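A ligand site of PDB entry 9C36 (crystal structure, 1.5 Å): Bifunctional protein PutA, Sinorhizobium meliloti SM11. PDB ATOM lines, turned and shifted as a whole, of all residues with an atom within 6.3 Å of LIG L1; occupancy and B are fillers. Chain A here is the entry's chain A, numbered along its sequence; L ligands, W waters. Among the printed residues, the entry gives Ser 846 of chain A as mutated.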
ATOM      1  N   GLU A 676     -13.091 -39.595  -8.228  1.00  0.00           N
ATOM      2  CA  GLU A 676     -14.359 -39.527  -8.968  1.00  0.00           C
ATOM      3  C   GLU A 676     -14.246 -40.260 -10.299  1.00  0.00           C
ATOM      4  O   GLU A 676     -15.185 -40.942 -10.716  1.00  0.00           O
ATOM      5  CB  GLU A 676     -14.743 -38.070  -9.185  1.00  0.00           C
ATOM      6  CG  GLU A 676     -16.089 -37.884  -9.849  1.00  0.00           C
ATOM      7  CD  GLU A 676     -16.581 -36.442  -9.781  1.00  0.00           C
ATOM      8  OE1 GLU A 676     -15.983 -35.638  -9.045  1.00  0.00           O
ATOM      9  OE2 GLU A 676     -17.586 -36.117 -10.455  1.00  0.00           O
ATOM     10  N   ASN A 709     -12.719 -28.049 -16.233  1.00  0.00           N
ATOM     11  CA  ASN A 709     -12.566 -27.877 -14.787  1.00  0.00           C
ATOM     12  C   ASN A 709     -12.575 -29.164 -13.999  1.00  0.00           C
ATOM     13  O   ASN A 709     -12.153 -29.162 -12.828  1.00  0.00           O
ATOM     14  CB  ASN A 709     -13.638 -26.947 -14.237  1.00  0.00           C
ATOM     15  CG  ASN A 709     -14.999 -27.537 -14.324  1.00  0.00           C
ATOM     16  OD1 ASN A 709     -15.424 -27.971 -15.390  1.00  0.00           O
ATOM     17  ND2 ASN A 709     -15.679 -27.595 -13.190  1.00  0.00           N
ATOM     18  N   PHE A 710     -13.071 -30.253 -14.555  1.00  0.00           N
ATOM     19  CA  PHE A 710     -12.849 -31.596 -14.043  1.00  0.00           C
ATOM     20  C   PHE A 710     -12.308 -32.397 -15.210  1.00  0.00           C
ATOM     21  O   PHE A 710     -13.013 -33.233 -15.808  1.00  0.00           O
ATOM     22  CB  PHE A 710     -14.086 -32.216 -13.416  1.00  0.00           C
ATOM     23  CG  PHE A 710     -14.236 -31.829 -11.998  1.00  0.00           C
ATOM     24  CD1 PHE A 710     -14.801 -30.621 -11.652  1.00  0.00           C
ATOM     25  CD2 PHE A 710     -13.740 -32.647 -10.994  1.00  0.00           C
ATOM     26  CE1 PHE A 710     -14.915 -30.251 -10.329  1.00  0.00           C
ATOM     27  CE2 PHE A 710     -13.854 -32.277  -9.671  1.00  0.00           C
ATOM     28  CZ  PHE A 710     -14.445 -31.074  -9.343  1.00  0.00           C
ATOM     29  N   ILE A 714     -14.937 -35.760 -15.295  1.00  0.00           N
ATOM     30  CA  ILE A 714     -16.096 -35.610 -16.174  1.00  0.00           C
ATOM     31  C   ILE A 714     -15.759 -36.173 -17.541  1.00  0.00           C
ATOM     32  O   ILE A 714     -16.582 -36.848 -18.180  1.00  0.00           O
ATOM     33  CB  ILE A 714     -16.529 -34.152 -16.233  1.00  0.00           C
ATOM     34  CG1 ILE A 714     -17.071 -33.727 -14.848  1.00  0.00           C
ATOM     35  CG2 ILE A 714     -17.556 -33.948 -17.367  1.00  0.00           C
ATOM     36  CD1 ILE A 714     -17.581 -32.281 -14.763  1.00  0.00           C
ATOM     37  N   GLN A 844     -14.410 -22.742  -9.428  1.00  0.00           N
ATOM     38  CA  GLN A 844     -14.512 -23.312 -10.767  1.00  0.00           C
ATOM     39  C   GLN A 844     -15.101 -24.728 -10.692  1.00  0.00           C
ATOM     40  O   GLN A 844     -14.504 -25.732 -11.129  1.00  0.00           O
ATOM     41  CB  GLN A 844     -13.178 -23.229 -11.479  1.00  0.00           C
ATOM     42  CG  GLN A 844     -12.743 -21.787 -11.656  1.00  0.00           C
ATOM     43  CD  GLN A 844     -11.293 -21.665 -12.104  1.00  0.00           C
ATOM     44  OE1 GLN A 844     -11.000 -21.138 -13.184  1.00  0.00           O
ATOM     45  NE2 GLN A 844     -10.388 -22.171 -11.300  1.00  0.00           N
ATOM     46  N   ARG A 845     -16.263 -24.785 -10.063  1.00  0.00           N
ATOM     47  CA  ARG A 845     -17.114 -25.963 -10.035  1.00  0.00           C
ATOM     48  C   ARG A 845     -18.503 -25.529 -10.448  1.00  0.00           C
ATOM     49  O   ARG A 845     -18.993 -24.473 -10.031  1.00  0.00           O
ATOM     50  CB  ARG A 845     -17.261 -26.535  -8.638  1.00  0.00           C
ATOM     51  CG  ARG A 845     -15.994 -27.131  -8.064  1.00  0.00           C
ATOM     52  CD  ARG A 845     -16.360 -27.734  -6.717  1.00  0.00           C
ATOM     53  NE  ARG A 845     -15.193 -28.226  -6.008  1.00  0.00           N
ATOM     54  CZ  ARG A 845     -14.910 -29.516  -5.817  1.00  0.00           C
ATOM     55  NH1 ARG A 845     -15.704 -30.487  -6.253  1.00  0.00           N
ATOM     56  NH2 ARG A 845     -13.807 -29.840  -5.150  1.00  0.00           N
ATOM     57  N   SER A 846     -19.177 -26.380 -11.212  1.00  0.00           N
ATOM     58  CA  SER A 846     -20.536 -26.042 -11.602  1.00  0.00           C
ATOM     59  C   SER A 846     -21.415 -25.949 -10.380  1.00  0.00           C
ATOM     60  O   SER A 846     -22.363 -25.181 -10.367  1.00  0.00           O
ATOM     61  CB  SER A 846     -21.071 -27.104 -12.559  1.00  0.00           C
ATOM     62  OG  SER A 846     -21.239 -28.339 -11.909  1.00  0.00           O
ATOM     63  N   SER A 847     -21.067 -26.715  -9.350  1.00  0.00           N
ATOM     64  CA  SER A 847     -21.795 -26.810  -8.093  1.00  0.00           C
ATOM     65  C   SER A 847     -21.466 -25.688  -7.124  1.00  0.00           C
ATOM     66  O   SER A 847     -22.060 -25.640  -6.034  1.00  0.00           O
ATOM     67  CB  SER A 847     -21.420 -28.141  -7.445  1.00  0.00           C
ATOM     68  OG  SER A 847     -19.997 -28.199  -7.308  1.00  0.00           O
ATOM     69  N   ALA A 848     -20.505 -24.822  -7.446  1.00  0.00           N
ATOM     70  CA  ALA A 848     -19.986 -23.910  -6.436  1.00  0.00           C
ATOM     71  C   ALA A 848     -21.053 -22.937  -5.948  1.00  0.00           C
ATOM     72  O   ALA A 848     -21.979 -22.571  -6.655  1.00  0.00           O
ATOM     73  CB  ALA A 848     -18.797 -23.113  -7.000  1.00  0.00           C
ATOM     74  N   PHE A 944     -18.165 -17.903 -13.289  1.00  0.00           N
ATOM     75  CA  PHE A 944     -17.461 -19.147 -12.991  1.00  0.00           C
ATOM     76  C   PHE A 944     -16.098 -18.800 -12.429  1.00  0.00           C
ATOM     77  O   PHE A 944     -15.061 -18.881 -13.108  1.00  0.00           O
ATOM     78  CB  PHE A 944     -17.342 -19.980 -14.263  1.00  0.00           C
ATOM     79  CG  PHE A 944     -17.103 -21.435 -14.003  1.00  0.00           C
ATOM     80  CD1 PHE A 944     -18.078 -22.213 -13.408  1.00  0.00           C
ATOM     81  CD2 PHE A 944     -15.910 -22.042 -14.389  1.00  0.00           C
ATOM     82  CE1 PHE A 944     -17.853 -23.564 -13.186  1.00  0.00           C
ATOM     83  CE2 PHE A 944     -15.708 -23.394 -14.161  1.00  0.00           C
ATOM     84  CZ  PHE A 944     -16.667 -24.152 -13.550  1.00  0.00           C
ATOM     85  N   LEU A 972     -29.162 -26.308 -10.261  1.00  0.00           N
ATOM     86  CA  LEU A 972     -28.095 -27.282 -10.101  1.00  0.00           C
ATOM     87  C   LEU A 972     -27.953 -27.704  -8.634  1.00  0.00           C
ATOM     88  O   LEU A 972     -28.556 -28.692  -8.221  1.00  0.00           O
ATOM     89  CB  LEU A 972     -26.802 -26.795 -10.747  1.00  0.00           C
ATOM     90  CG  LEU A 972     -25.725 -27.859 -10.847  1.00  0.00           C
ATOM     91  CD1 LEU A 972     -26.193 -29.192 -11.447  1.00  0.00           C
ATOM     92  CD2 LEU A 972     -24.593 -27.335 -11.741  1.00  0.00           C
ATOM     93  N   THR A 973     -27.141 -26.997  -7.851  1.00  0.00           N
ATOM     94  CA  THR A 973     -27.002 -27.325  -6.450  1.00  0.00           C
ATOM     95  C   THR A 973     -27.688 -26.266  -5.605  1.00  0.00           C
ATOM     96  O   THR A 973     -27.863 -25.113  -6.008  1.00  0.00           O
ATOM     97  CB  THR A 973     -25.524 -27.458  -6.042  1.00  0.00           C
ATOM     98  OG1 THR A 973     -24.874 -26.218  -6.299  1.00  0.00           O
ATOM     99  CG2 THR A 973     -24.839 -28.610  -6.838  1.00  0.00           C
ATOM    100  N   TYR A 997     -28.504 -30.086  -0.486  1.00  0.00           N
ATOM    101  CA  TYR A 997     -27.574 -30.382   0.584  1.00  0.00           C
ATOM    102  C   TYR A 997     -28.040 -29.676   1.828  1.00  0.00           C
ATOM    103  O   TYR A 997     -28.301 -28.470   1.795  1.00  0.00           O
ATOM    104  CB  TYR A 997     -26.170 -29.885   0.211  1.00  0.00           C
ATOM    105  CG  TYR A 997     -25.630 -30.510  -1.049  1.00  0.00           C
ATOM    106  CD1 TYR A 997     -24.974 -31.714  -1.015  1.00  0.00           C
ATOM    107  CD2 TYR A 997     -25.806 -29.884  -2.266  1.00  0.00           C
ATOM    108  CE1 TYR A 997     -24.500 -32.273  -2.177  1.00  0.00           C
ATOM    109  CE2 TYR A 997     -25.335 -30.437  -3.421  1.00  0.00           C
ATOM    110  CZ  TYR A 997     -24.677 -31.622  -3.362  1.00  0.00           C
ATOM    111  OH  TYR A 997     -24.187 -32.246  -4.518  1.00  0.00           O
ATOM    112  N   ILE A1002     -22.074 -27.770  -0.539  1.00  0.00           N
ATOM    113  CA  ILE A1002     -22.905 -28.074  -1.706  1.00  0.00           C
ATOM    114  C   ILE A1002     -22.090 -28.610  -2.863  1.00  0.00           C
ATOM    115  O   ILE A1002     -22.577 -28.608  -4.005  1.00  0.00           O
ATOM    116  CB  ILE A1002     -23.783 -26.882  -2.116  1.00  0.00           C
ATOM    117  CG1 ILE A1002     -22.980 -25.712  -2.667  1.00  0.00           C
ATOM    118  CG2 ILE A1002     -24.638 -26.440  -0.948  1.00  0.00           C
ATOM    119  CD1 ILE A1002     -23.873 -24.674  -3.278  1.00  0.00           C
ATOM    120  N   ILE A1003     -20.882 -29.129  -2.577  1.00  0.00           N
ATOM    121  CA  ILE A1003     -19.917 -29.502  -3.603  1.00  0.00           C
ATOM    122  C   ILE A1003     -19.358 -30.909  -3.365  1.00  0.00           C
ATOM    123  O   ILE A1003     -19.543 -31.523  -2.324  1.00  0.00           O
ATOM    124  CB  ILE A1003     -18.751 -28.489  -3.720  1.00  0.00           C
ATOM    125  CG1 ILE A1003     -17.919 -28.449  -2.440  1.00  0.00           C
ATOM    126  CG2 ILE A1003     -19.262 -27.101  -4.086  1.00  0.00           C
ATOM    127  CD1 ILE A1003     -16.477 -27.970  -2.664  1.00  0.00           C
ATOM    128  N   GLY A1004     -18.634 -31.402  -4.361  1.00  0.00           N
ATOM    129  CA  GLY A1004     -18.064 -32.729  -4.255  1.00  0.00           C
ATOM    130  C   GLY A1004     -19.104 -33.837  -4.284  1.00  0.00           C
ATOM    131  O   GLY A1004     -18.979 -34.812  -3.534  1.00  0.00           O
ATOM    132  N   ALA A1005     -20.110 -33.709  -5.144  1.00  0.00           N
ATOM    133  CA  ALA A1005     -21.083 -34.781  -5.288  1.00  0.00           C
ATOM    134  C   ALA A1005     -20.366 -36.068  -5.676  1.00  0.00           C
ATOM    135  O   ALA A1005     -19.425 -36.061  -6.488  1.00  0.00           O
ATOM    136  CB  ALA A1005     -22.115 -34.434  -6.367  1.00  0.00           C
ATOM    137  N   VAL A1006     -20.800 -37.164  -5.073  1.00  0.00           N
ATOM    138  CA  VAL A1006     -20.114 -38.446  -5.153  1.00  0.00           C
ATOM    139  C   VAL A1006     -20.937 -39.386  -6.016  1.00  0.00           C
ATOM    140  O   VAL A1006     -22.162 -39.468  -5.873  1.00  0.00           O
ATOM    141  CB  VAL A1006     -19.916 -39.025  -3.738  1.00  0.00           C
ATOM    142  CG1 VAL A1006     -19.388 -40.458  -3.814  1.00  0.00           C
ATOM    143  CG2 VAL A1006     -18.978 -38.121  -2.927  1.00  0.00           C
ATOM    144  N   PHE A1012     -25.370 -36.584  -9.800  1.00  0.00           N
ATOM    145  CA  PHE A1012     -25.163 -35.166  -9.969  1.00  0.00           C
ATOM    146  C   PHE A1012     -25.789 -34.677 -11.255  1.00  0.00           C
ATOM    147  O   PHE A1012     -25.542 -35.255 -12.331  1.00  0.00           O
ATOM    148  CB  PHE A1012     -23.677 -34.837  -9.957  1.00  0.00           C
ATOM    149  CG  PHE A1012     -23.420 -33.373  -9.972  1.00  0.00           C
ATOM    150  CD1 PHE A1012     -23.604 -32.618  -8.819  1.00  0.00           C
ATOM    151  CD2 PHE A1012     -23.076 -32.727 -11.147  1.00  0.00           C
ATOM    152  CE1 PHE A1012     -23.427 -31.255  -8.831  1.00  0.00           C
ATOM    153  CE2 PHE A1012     -22.871 -31.365 -11.148  1.00  0.00           C
ATOM    154  CZ  PHE A1012     -23.033 -30.631  -9.997  1.00  0.00           C
HETATM  155  N1  LIG L   1     -20.028 -32.731  -9.560  1.00  0.00           N
HETATM  156  C1  LIG L   1     -19.166 -31.632  -9.235  1.00  0.00           C
HETATM  157  C2  LIG L   1     -19.291 -31.215  -7.765  1.00  0.00           C
HETATM  158  C3  LIG L   1     -19.601 -30.448 -10.078  1.00  0.00           C
HETATM  159  C4  LIG L   1     -18.987 -30.596 -11.454  1.00  0.00           C
HETATM  160  C5  LIG L   1     -18.023 -29.429 -11.501  1.00  0.00           C
HETATM  161  O1  LIG L   1     -18.215 -28.522 -12.109  1.00  0.00           O
HETATM  162  O2  LIG L   1     -20.304 -31.524  -7.104  1.00  0.00           O
HETATM  163  O3  LIG L   1     -18.373 -30.562  -7.238  1.00  0.00           O
HETATM  164  P1  LG2 L   2     -17.262 -24.449 -22.233  1.00  0.00           P
HETATM  165  O1  LG2 L   2     -18.764 -24.309 -22.520  1.00  0.00           O
HETATM  166  O2  LG2 L   2     -16.458 -23.266 -22.362  1.00  0.00           O
HETATM  167  O3  LG2 L   2     -16.526 -25.534 -22.986  1.00  0.00           O
HETATM  168  C1  LG2 L   2     -16.918 -26.870 -22.801  1.00  0.00           C
HETATM  169  C2  LG2 L   2     -16.514 -27.772 -23.957  1.00  0.00           C
HETATM  170  O4  LG2 L   2     -17.301 -27.449 -25.120  1.00  0.00           O
HETATM  171  C3  LG2 L   2     -15.069 -27.708 -24.399  1.00  0.00           C
HETATM  172  O5  LG2 L   2     -14.634 -28.984 -24.720  1.00  0.00           O
HETATM  173  C4  LG2 L   2     -15.092 -26.764 -25.533  1.00  0.00           C
HETATM  174  O6  LG2 L   2     -14.011 -26.932 -26.366  1.00  0.00           O
HETATM  175  C5  LG2 L   2     -16.364 -27.171 -26.174  1.00  0.00           C
HETATM  176  N1  LG2 L   2     -16.947 -26.223 -27.073  1.00  0.00           N
HETATM  177  C6  LG2 L   2     -16.842 -24.866 -27.038  1.00  0.00           C
HETATM  178  N2  LG2 L   2     -17.542 -24.317 -28.009  1.00  0.00           N
HETATM  179  C7  LG2 L   2     -18.144 -25.319 -28.756  1.00  0.00           C
HETATM  180  C8  LG2 L   2     -18.978 -25.374 -29.863  1.00  0.00           C
HETATM  181  N3  LG2 L   2     -19.373 -24.166 -30.497  1.00  0.00           N
HETATM  182  N4  LG2 L   2     -19.389 -26.554 -30.315  1.00  0.00           N
HETATM  183  C9  LG2 L   2     -19.029 -27.725 -29.751  1.00  0.00           C
HETATM  184  N5  LG2 L   2     -18.214 -27.726 -28.658  1.00  0.00           N
HETATM  185  C10 LG2 L   2     -17.778 -26.558 -28.161  1.00  0.00           C
HETATM  186  O7  LG2 L   2     -17.063 -24.869 -20.775  1.00  0.00           O
HETATM  187  P2  LG2 L   2     -15.807 -24.944 -19.804  1.00  0.00           P
HETATM  188  O8  LG2 L   2     -15.323 -23.544 -19.579  1.00  0.00           O
HETATM  189  O9  LG2 L   2     -14.803 -25.924 -20.295  1.00  0.00           O
HETATM  190  O10 LG2 L   2     -16.434 -25.483 -18.412  1.00  0.00           O
HETATM  191  C11 LG2 L   2     -17.050 -24.600 -17.516  1.00  0.00           C
HETATM  192  C12 LG2 L   2     -18.582 -24.646 -17.632  1.00  0.00           C
HETATM  193  O11 LG2 L   2     -18.997 -25.991 -17.610  1.00  0.00           O
HETATM  194  C13 LG2 L   2     -19.266 -23.940 -16.517  1.00  0.00           C
HETATM  195  O12 LG2 L   2     -20.343 -23.209 -17.016  1.00  0.00           O
HETATM  196  C14 LG2 L   2     -19.750 -25.027 -15.642  1.00  0.00           C
HETATM  197  O13 LG2 L   2     -20.819 -24.634 -14.845  1.00  0.00           O
HETATM  198  C15 LG2 L   2     -20.024 -26.078 -16.666  1.00  0.00           C
HETATM  199  N6  LG2 L   2     -19.967 -27.358 -16.049  1.00  0.00           N
HETATM  200  C16 LG2 L   2     -21.142 -28.060 -15.736  1.00  0.00           C
HETATM  201  C17 LG2 L   2     -21.026 -29.273 -15.073  1.00  0.00           C
HETATM  202  C18 LG2 L   2     -22.241 -30.042 -14.745  1.00  0.00           C
HETATM  203  O14 LG2 L   2     -22.156 -31.207 -14.416  1.00  0.00           O
HETATM  204  N7  LG2 L   2     -23.472 -29.371 -14.815  1.00  0.00           N
HETATM  205  C19 LG2 L   2     -19.767 -29.817 -14.694  1.00  0.00           C
HETATM  206  C20 LG2 L   2     -18.615 -29.099 -15.030  1.00  0.00           C
HETATM  207  C21 LG2 L   2     -18.706 -27.866 -15.673  1.00  0.00           C
HETATM  208  O   HOH W   1     -22.449 -30.852  -5.618  1.00  0.00           O
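N of Ser 846 is in hydrogen-bond range of O1 of LIG L1 (2.5 Å).
The side-chain hydroxyl (OG) of Ser 846 lies within hydrogen-bond range of an oxygen (O1) of LIG L1 (3.0 Å).
NH1 of Arg 845 lies within salt-bridge range of O3 of LIG L1, 2.8 Å away.
The side-chain hydroxyl of Ser 847 lies within hydrogen-bond range of an oxygen (O3) of LIG L1 (2.9 Å).
O1 of LIG L1 is in hydrogen-bond range of ND2 of Asn 709 (2.9 Å).
The backbone NH (N) of Ala 1005 sits at hydrogen-bond distance from an oxygen (O2) of LIG L1.
The backbone NH (N) of Gly 1004 lies within hydrogen-bond range of an oxygen (O3) of LIG L1, 3.0 Å away.
O of Ser 847 sits at hydrogen-bond distance from OG1 of Thr 973.
O of Gln 844 is in hydrogen-bond range of ND2 of Asn 709 (3.0 Å).
Phe 710 touches LIG L1.
Ile 714 touches LIG L1.
Ile 1003 touches LIG L1.
Phe 1012 touches LIG L1 (CD2 to N1, 3.4 Å).
Hydrophobic or aromatic side chains within 4 Å of LIG L1: Phe 710, Ile 714, Ala 1005 and Phe 1012.
Within 4 Å of LIG L1: Asn 709, Phe 710, Ile 714, Arg 845, Ser 846, Ser 847, Ile 1003, Gly 1004, Ala 1005 and Phe 1012.
The nearest printed residue that does not touch LIG L1 is Glu 676 (4.3 Å).
Water W1 lies within hydrogen-bond range of the side-chain hydroxyl (OH) of Tyr 997 (2.5 Å), an oxygen (O2) of LIG L1 (2.7 Å) and the backbone carbonyl oxygen (O) of Ile 1002 (2.8 Å).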
